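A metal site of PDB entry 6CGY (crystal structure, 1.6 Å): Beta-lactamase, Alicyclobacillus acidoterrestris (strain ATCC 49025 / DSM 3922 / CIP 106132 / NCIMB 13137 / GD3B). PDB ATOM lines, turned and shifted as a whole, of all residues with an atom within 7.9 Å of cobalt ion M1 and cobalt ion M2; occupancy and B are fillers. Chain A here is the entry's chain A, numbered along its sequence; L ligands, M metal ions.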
ATOM      1  N   MET A  19      -1.759 -27.009   5.880  1.00  0.00           N
ATOM      2  CA  MET A  19      -1.604 -26.049   4.803  1.00  0.00           C
ATOM      3  C   MET A  19      -1.281 -26.826   3.531  1.00  0.00           C
ATOM      4  O   MET A  19      -0.700 -27.911   3.570  1.00  0.00           O
ATOM      5  CB  MET A  19      -0.451 -25.077   5.118  1.00  0.00           C
ATOM      6  CG  MET A  19      -0.159 -24.033   4.085  1.00  0.00           C
ATOM      7  SD  MET A  19       1.039 -22.819   4.713  1.00  0.00           S
ATOM      8  CE  MET A  19       0.100 -22.218   6.122  1.00  0.00           C
ATOM      9  N   MET A  21       0.399 -26.253  -0.521  1.00  0.00           N
ATOM     10  CA  MET A  21       1.110 -25.355  -1.410  1.00  0.00           C
ATOM     11  C   MET A  21       1.839 -26.137  -2.484  1.00  0.00           C
ATOM     12  O   MET A  21       1.989 -27.352  -2.371  1.00  0.00           O
ATOM     13  CB  MET A  21       2.129 -24.512  -0.637  1.00  0.00           C
ATOM     14  CG  MET A  21       3.363 -25.277  -0.172  1.00  0.00           C
ATOM     15  SD  MET A  21       4.312 -24.189   0.919  1.00  0.00           S
ATOM     16  CE  MET A  21       5.660 -25.291   1.361  1.00  0.00           C
ATOM     17  N   PHE A  47       0.685 -30.285   4.340  1.00  0.00           N
ATOM     18  CA  PHE A  47       1.616 -30.466   5.444  1.00  0.00           C
ATOM     19  C   PHE A  47       1.053 -29.888   6.722  1.00  0.00           C
ATOM     20  O   PHE A  47       0.138 -29.067   6.681  1.00  0.00           O
ATOM     21  CB  PHE A  47       2.973 -29.839   5.098  1.00  0.00           C
ATOM     22  CG  PHE A  47       2.887 -28.397   4.720  1.00  0.00           C
ATOM     23  CD1 PHE A  47       3.017 -27.407   5.675  1.00  0.00           C
ATOM     24  CD2 PHE A  47       2.712 -28.021   3.390  1.00  0.00           C
ATOM     25  CE1 PHE A  47       2.940 -26.083   5.313  1.00  0.00           C
ATOM     26  CE2 PHE A  47       2.625 -26.694   3.029  1.00  0.00           C
ATOM     27  CZ  PHE A  47       2.741 -25.720   3.996  1.00  0.00           C
ATOM     28  N   PRO A  48       1.578 -30.311   7.864  1.00  0.00           N
ATOM     29  CA  PRO A  48       1.011 -29.877   9.129  1.00  0.00           C
ATOM     30  C   PRO A  48       1.611 -28.557   9.626  1.00  0.00           C
ATOM     31  O   PRO A  48       2.778 -28.268   9.338  1.00  0.00           O
ATOM     32  CB  PRO A  48       1.378 -31.008  10.083  1.00  0.00           C
ATOM     33  CG  PRO A  48       2.643 -31.558   9.540  1.00  0.00           C
ATOM     34  CD  PRO A  48       2.661 -31.305   8.051  1.00  0.00           C
ATOM     35  N   ILE A  49       0.801 -27.818  10.366  1.00  0.00           N
ATOM     36  CA  ILE A  49       1.208 -26.622  11.118  1.00  0.00           C
ATOM     37  C   ILE A  49       1.068 -27.016  12.570  1.00  0.00           C
ATOM     38  O   ILE A  49       0.005 -27.470  12.981  1.00  0.00           O
ATOM     39  CB  ILE A  49       0.277 -25.435  10.835  1.00  0.00           C
ATOM     40  CG1 ILE A  49       0.158 -25.141   9.334  1.00  0.00           C
ATOM     41  CG2 ILE A  49       0.709 -24.205  11.614  1.00  0.00           C
ATOM     42  CD1 ILE A  49       1.468 -25.070   8.588  1.00  0.00           C
ATOM     43  N   ASP A  64       6.742 -21.448  18.734  1.00  0.00           N
ATOM     44  CA  ASP A  64       5.858 -21.062  17.598  1.00  0.00           C
ATOM     45  C   ASP A  64       4.405 -20.906  18.036  1.00  0.00           C
ATOM     46  O   ASP A  64       4.026 -21.275  19.156  1.00  0.00           O
ATOM     47  CB  ASP A  64       5.953 -22.041  16.412  1.00  0.00           C
ATOM     48  CG  ASP A  64       7.208 -21.829  15.566  1.00  0.00           C
ATOM     49  OD1 ASP A  64       7.844 -20.757  15.659  1.00  0.00           O
ATOM     50  OD2 ASP A  64       7.542 -22.759  14.784  1.00  0.00           O
ATOM     51  N   SER A 116      10.221 -18.796  16.068  1.00  0.00           N
ATOM     52  CA  SER A 116      11.299 -19.356  15.267  1.00  0.00           C
ATOM     53  C   SER A 116      11.624 -18.407  14.147  1.00  0.00           C
ATOM     54  O   SER A 116      12.798 -18.258  13.764  1.00  0.00           O
ATOM     55  CB  SER A 116      10.937 -20.729  14.697  1.00  0.00           C
ATOM     56  OG  SER A 116       9.820 -20.697  13.806  1.00  0.00           O
ATOM     57  N   HIS A 117      10.574 -17.825  13.583  1.00  0.00           N
ATOM     58  CA  HIS A 117      10.651 -16.725  12.630  1.00  0.00           C
ATOM     59  C   HIS A 117       9.273 -16.098  12.564  1.00  0.00           C
ATOM     60  O   HIS A 117       8.371 -16.554  13.308  1.00  0.00           O
ATOM     61  CB  HIS A 117      11.213 -17.159  11.254  1.00  0.00           C
ATOM     62  CG  HIS A 117      10.430 -18.228  10.555  1.00  0.00           C
ATOM     63  ND1 HIS A 117      10.030 -19.393  11.156  1.00  0.00           N
ATOM     64  CD2 HIS A 117      10.059 -18.335   9.260  1.00  0.00           C
ATOM     65  CE1 HIS A 117       9.438 -20.168  10.267  1.00  0.00           C
ATOM     66  NE2 HIS A 117       9.435 -19.549   9.112  1.00  0.00           N
ATOM     67  N   LEU A 118       9.080 -15.081  11.746  1.00  0.00           N
ATOM     68  CA  LEU A 118       7.836 -14.305  11.787  1.00  0.00           C
ATOM     69  C   LEU A 118       6.904 -14.533  10.593  1.00  0.00           C
ATOM     70  O   LEU A 118       6.017 -13.724  10.326  1.00  0.00           O
ATOM     71  CB  LEU A 118       8.121 -12.810  11.987  1.00  0.00           C
ATOM     72  CG  LEU A 118       8.755 -12.490  13.344  1.00  0.00           C
ATOM     73  CD1 LEU A 118       9.126 -11.022  13.461  1.00  0.00           C
ATOM     74  CD2 LEU A 118       7.873 -12.913  14.530  1.00  0.00           C
ATOM     75  N   HIS A 119       7.071 -15.682   9.929  1.00  0.00           N
ATOM     76  CA  HIS A 119       6.161 -16.112   8.878  1.00  0.00           C
ATOM     77  C   HIS A 119       4.734 -16.350   9.383  1.00  0.00           C
ATOM     78  O   HIS A 119       4.532 -16.645  10.553  1.00  0.00           O
ATOM     79  CB  HIS A 119       6.672 -17.366   8.186  1.00  0.00           C
ATOM     80  CG  HIS A 119       7.720 -17.095   7.156  1.00  0.00           C
ATOM     81  ND1 HIS A 119       8.488 -18.079   6.577  1.00  0.00           N
ATOM     82  CD2 HIS A 119       8.125 -15.931   6.596  1.00  0.00           C
ATOM     83  CE1 HIS A 119       9.311 -17.539   5.695  1.00  0.00           C
ATOM     84  NE2 HIS A 119       9.112 -16.224   5.692  1.00  0.00           N
ATOM     85  N   LEU A 120       3.802 -16.217   8.460  1.00  0.00           N
ATOM     86  CA  LEU A 120       2.365 -16.299   8.698  1.00  0.00           C
ATOM     87  C   LEU A 120       1.907 -17.506   9.506  1.00  0.00           C
ATOM     88  O   LEU A 120       0.929 -17.426  10.263  1.00  0.00           O
ATOM     89  CB  LEU A 120       1.622 -16.253   7.354  1.00  0.00           C
ATOM     90  CG  LEU A 120       1.735 -17.432   6.363  1.00  0.00           C
ATOM     91  CD1 LEU A 120       0.917 -17.152   5.095  1.00  0.00           C
ATOM     92  CD2 LEU A 120       3.163 -17.757   5.965  1.00  0.00           C
ATOM     93  N   ASP A 121       2.621 -18.624   9.366  1.00  0.00           N
ATOM     94  CA  ASP A 121       2.218 -19.882   9.994  1.00  0.00           C
ATOM     95  C   ASP A 121       2.986 -20.230  11.277  1.00  0.00           C
ATOM     96  O   ASP A 121       2.804 -21.315  11.820  1.00  0.00           O
ATOM     97  CB  ASP A 121       2.393 -21.028   8.996  1.00  0.00           C
ATOM     98  CG  ASP A 121       3.799 -21.109   8.435  1.00  0.00           C
ATOM     99  OD1 ASP A 121       4.400 -20.042   8.129  1.00  0.00           O
ATOM    100  OD2 ASP A 121       4.313 -22.229   8.300  1.00  0.00           O
ATOM    101  N   HIS A 122       3.840 -19.311  11.751  1.00  0.00           N
ATOM    102  CA  HIS A 122       4.581 -19.495  13.011  1.00  0.00           C
ATOM    103  C   HIS A 122       4.316 -18.363  14.001  1.00  0.00           C
ATOM    104  O   HIS A 122       4.403 -18.558  15.206  1.00  0.00           O
ATOM    105  CB  HIS A 122       6.073 -19.629  12.731  1.00  0.00           C
ATOM    106  CG  HIS A 122       6.388 -20.764  11.805  1.00  0.00           C
ATOM    107  ND1 HIS A 122       6.836 -21.990  12.262  1.00  0.00           N
ATOM    108  CD2 HIS A 122       6.249 -20.890  10.468  1.00  0.00           C
ATOM    109  CE1 HIS A 122       6.969 -22.810  11.226  1.00  0.00           C
ATOM    110  NE2 HIS A 122       6.614 -22.166  10.138  1.00  0.00           N
ATOM    111  N   GLU A 140      15.157 -10.766  12.037  1.00  0.00           N
ATOM    112  CA  GLU A 140      13.843 -11.210  11.604  1.00  0.00           C
ATOM    113  C   GLU A 140      12.787 -10.161  12.020  1.00  0.00           C
ATOM    114  O   GLU A 140      11.877  -9.814  11.240  1.00  0.00           O
ATOM    115  CB  GLU A 140      13.561 -12.599  12.183  1.00  0.00           C
ATOM    116  CG  GLU A 140      12.212 -13.168  11.772  1.00  0.00           C
ATOM    117  CD  GLU A 140      12.145 -13.621  10.318  1.00  0.00           C
ATOM    118  OE1 GLU A 140      13.180 -13.612   9.627  1.00  0.00           O
ATOM    119  OE2 GLU A 140      11.041 -14.015   9.848  1.00  0.00           O
ATOM    120  N   ALA A 156       4.384 -13.484   2.990  1.00  0.00           N
ATOM    121  CA  ALA A 156       4.509 -14.338   4.174  1.00  0.00           C
ATOM    122  C   ALA A 156       4.518 -13.598   5.492  1.00  0.00           C
ATOM    123  O   ALA A 156       4.434 -14.214   6.548  1.00  0.00           O
ATOM    124  CB  ALA A 156       5.785 -15.156   4.077  1.00  0.00           C
ATOM    125  N   TYR A 157       4.662 -12.274   5.434  1.00  0.00           N
ATOM    126  CA  TYR A 157       4.612 -11.466   6.630  1.00  0.00           C
ATOM    127  C   TYR A 157       3.291 -10.719   6.640  1.00  0.00           C
ATOM    128  O   TYR A 157       3.028  -9.901   5.756  1.00  0.00           O
ATOM    129  CB  TYR A 157       5.827 -10.548   6.673  1.00  0.00           C
ATOM    130  CG  TYR A 157       7.111 -11.333   6.858  1.00  0.00           C
ATOM    131  CD1 TYR A 157       7.490 -11.804   8.119  1.00  0.00           C
ATOM    132  CD2 TYR A 157       7.912 -11.635   5.777  1.00  0.00           C
ATOM    133  CE1 TYR A 157       8.651 -12.530   8.282  1.00  0.00           C
ATOM    134  CE2 TYR A 157       9.052 -12.387   5.922  1.00  0.00           C
ATOM    135  CZ  TYR A 157       9.417 -12.833   7.175  1.00  0.00           C
ATOM    136  OH  TYR A 157      10.560 -13.575   7.319  1.00  0.00           O
ATOM    137  N   HIS A 197      16.460 -19.691   5.620  1.00  0.00           N
ATOM    138  CA  HIS A 197      15.083 -19.688   5.196  1.00  0.00           C
ATOM    139  C   HIS A 197      14.467 -18.287   5.270  1.00  0.00           C
ATOM    140  O   HIS A 197      13.727 -17.888   4.378  1.00  0.00           O
ATOM    141  CB  HIS A 197      14.304 -20.670   6.082  1.00  0.00           C
ATOM    142  CG  HIS A 197      12.826 -20.578   5.947  1.00  0.00           C
ATOM    143  ND1 HIS A 197      12.144 -21.027   4.835  1.00  0.00           N
ATOM    144  CD2 HIS A 197      11.872 -20.118   6.799  1.00  0.00           C
ATOM    145  CE1 HIS A 197      10.850 -20.851   5.010  1.00  0.00           C
ATOM    146  NE2 HIS A 197      10.656 -20.302   6.199  1.00  0.00           N
ATOM    147  N   ALA A 198      14.777 -17.548   6.326  1.00  0.00           N
ATOM    148  CA  ALA A 198      14.313 -16.182   6.511  1.00  0.00           C
ATOM    149  C   ALA A 198      15.480 -15.336   7.043  1.00  0.00           C
ATOM    150  O   ALA A 198      16.628 -15.779   7.022  1.00  0.00           O
ATOM    151  CB  ALA A 198      13.127 -16.161   7.495  1.00  0.00           C
ATOM    152  N   MET A 201      16.598 -17.121  11.958  1.00  0.00           N
ATOM    153  CA  MET A 201      15.905 -18.336  12.384  1.00  0.00           C
ATOM    154  C   MET A 201      16.383 -18.751  13.774  1.00  0.00           C
ATOM    155  O   MET A 201      17.571 -18.868  13.998  1.00  0.00           O
ATOM    156  CB  MET A 201      16.181 -19.481  11.423  1.00  0.00           C
ATOM    157  CG  MET A 201      15.786 -19.217   9.977  1.00  0.00           C
ATOM    158  SD  MET A 201      14.031 -18.917   9.742  1.00  0.00           S
ATOM    159  CE  MET A 201      13.357 -20.503  10.207  1.00  0.00           C
ATOM    160  N   SER A 218      12.018 -25.994  13.270  1.00  0.00           N
ATOM    161  CA  SER A 218      11.075 -25.198  12.474  1.00  0.00           C
ATOM    162  C   SER A 218      11.498 -25.214  11.006  1.00  0.00           C
ATOM    163  O   SER A 218      11.984 -26.227  10.504  1.00  0.00           O
ATOM    164  CB  SER A 218      10.964 -23.775  13.027  1.00  0.00           C
ATOM    165  OG  SER A 218       9.967 -23.003  12.350  1.00  0.00           O
ATOM    166  N   ASP A 219      11.351 -24.083  10.336  1.00  0.00           N
ATOM    167  CA  ASP A 219      11.583 -24.010   8.884  1.00  0.00           C
ATOM    168  C   ASP A 219      13.049 -23.929   8.481  1.00  0.00           C
ATOM    169  O   ASP A 219      13.356 -23.801   7.293  1.00  0.00           O
ATOM    170  CB  ASP A 219      10.769 -22.874   8.272  1.00  0.00           C
ATOM    171  CG  ASP A 219       9.286 -23.144   8.289  1.00  0.00           C
ATOM    172  OD1 ASP A 219       8.880 -24.236   8.761  1.00  0.00           O
ATOM    173  OD2 ASP A 219       8.536 -22.276   7.813  1.00  0.00           O
ATOM    174  N   ALA A 220      13.969 -24.046   9.436  1.00  0.00           N
ATOM    175  CA  ALA A 220      15.355 -24.275   9.057  1.00  0.00           C
ATOM    176  C   ALA A 220      15.473 -25.629   8.333  1.00  0.00           C
ATOM    177  O   ALA A 220      16.377 -25.813   7.503  1.00  0.00           O
ATOM    178  CB  ALA A 220      16.263 -24.207  10.281  1.00  0.00           C
ATOM    179  N   TYR A 222      12.477 -28.062   6.562  1.00  0.00           N
ATOM    180  CA  TYR A 222      11.065 -28.305   6.348  1.00  0.00           C
ATOM    181  C   TYR A 222      10.678 -29.751   6.597  1.00  0.00           C
ATOM    182  O   TYR A 222       9.611 -30.045   7.155  1.00  0.00           O
ATOM    183  CB  TYR A 222      10.686 -27.994   4.912  1.00  0.00           C
ATOM    184  CG  TYR A 222      10.281 -26.570   4.556  1.00  0.00           C
ATOM    185  CD1 TYR A 222       9.692 -25.707   5.471  1.00  0.00           C
ATOM    186  CD2 TYR A 222      10.446 -26.129   3.253  1.00  0.00           C
ATOM    187  CE1 TYR A 222       9.278 -24.438   5.092  1.00  0.00           C
ATOM    188  CE2 TYR A 222      10.027 -24.879   2.874  1.00  0.00           C
ATOM    189  CZ  TYR A 222       9.443 -24.028   3.778  1.00  0.00           C
ATOM    190  OH  TYR A 222       9.024 -22.790   3.348  1.00  0.00           O
ATOM    191  N   GLY A 264      10.012 -28.659  10.555  1.00  0.00           N
ATOM    192  CA  GLY A 264       8.925 -27.691  10.549  1.00  0.00           C
ATOM    193  C   GLY A 264       7.607 -28.218  10.045  1.00  0.00           C
ATOM    194  O   GLY A 264       6.559 -27.943  10.623  1.00  0.00           O
ATOM    195  N   HIS A 265       7.646 -28.969   8.942  1.00  0.00           N
ATOM    196  CA  HIS A 265       6.432 -29.302   8.227  1.00  0.00           C
ATOM    197  C   HIS A 265       6.513 -30.697   7.557  1.00  0.00           C
ATOM    198  O   HIS A 265       6.299 -30.818   6.362  1.00  0.00           O
ATOM    199  CB  HIS A 265       6.154 -28.242   7.159  1.00  0.00           C
ATOM    200  CG  HIS A 265       5.929 -26.848   7.706  1.00  0.00           C
ATOM    201  ND1 HIS A 265       4.888 -26.538   8.566  1.00  0.00           N
ATOM    202  CD2 HIS A 265       6.566 -25.687   7.457  1.00  0.00           C
ATOM    203  CE1 HIS A 265       4.930 -25.251   8.844  1.00  0.00           C
ATOM    204  NE2 HIS A 265       5.932 -24.709   8.180  1.00  0.00           N
HETATM  205  P1  LIG L   1       6.581 -21.160   5.868  1.00  0.00           P
HETATM  206  O1  LIG L   1       6.333 -22.650   5.996  1.00  0.00           O
HETATM  207  O2  LIG L   1       6.631 -20.535   7.278  1.00  0.00           O
HETATM  208  O3  LIG L   1       7.914 -20.907   5.184  1.00  0.00           O
HETATM  209  O4  LIG L   1       5.465 -20.563   5.020  1.00  0.00           O
HETATM  210 CO    CO M   1       6.457 -22.665   8.058  1.00  0.00          CO
HETATM  211 CO    CO M   2       8.742 -20.155   7.130  1.00  0.00          CO
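The side-chain hydroxyl (OG) of Ser 218 lies close to a ring nitrogen (ND1) of His 122, 3.3 Å away.
O of Tyr 222 lies within hydrogen-bond range of N of His 265.
The side-chain hydroxyl (OH) of Tyr 157 lies within hydrogen-bond range of a ring nitrogen (NE2) of His 119 (3.4 Å).
A ring nitrogen (ND1) of His 117 lies within hydrogen-bond range of the side-chain hydroxyl (OG) of Ser 116 (3.0 Å).
The side-chain carboxylate (OD2) of Asp 64 lies within hydrogen-bond range of a ring nitrogen (ND1) of His 122 (2.7 Å).
ND1 of His 265 sits at hydrogen-bond distance from O of Pro 48.
Four residues have an atom within 4 Å of cobalt ion M1: Asp 121, His 122, Asp 219 and His 265.
The nearest printed residue that does not touch cobalt ion M1 is His 117 (4.4 Å).
Of the 25 residues printed, 4 come within 4 Å of cobalt ion M2.
The nearest printed residue that does not touch cobalt ion M2 is His 122 (4.2 Å).
O1 of the ligand is bound to cobalt ion M1 (2.1 Å).
NE2 of His 265 is bound to cobalt ion M1 (2.1 Å).
OD2 of Asp 219 is bound to cobalt ion M1 (2.1 Å).
NE2 of His 122 is bound to cobalt ion M1, at 2.1 Å.
The side-chain carboxylate (OD2) of Asp 121 is bound to cobalt ion M1, 2.2 Å away.
Cobalt ion M1 is bound by O2 of the ligand (2.3 Å).
Cobalt ion M2 is bound by NE2 of His 197 (2.1 Å), O2 of the ligand (2.2 Å), ND1 of His 119 (2.2 Å), NE2 of His 117 (2.2 Å), OD2 of Asp 219 (2.2 Å) and O3 of the ligand (2.2 Å).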
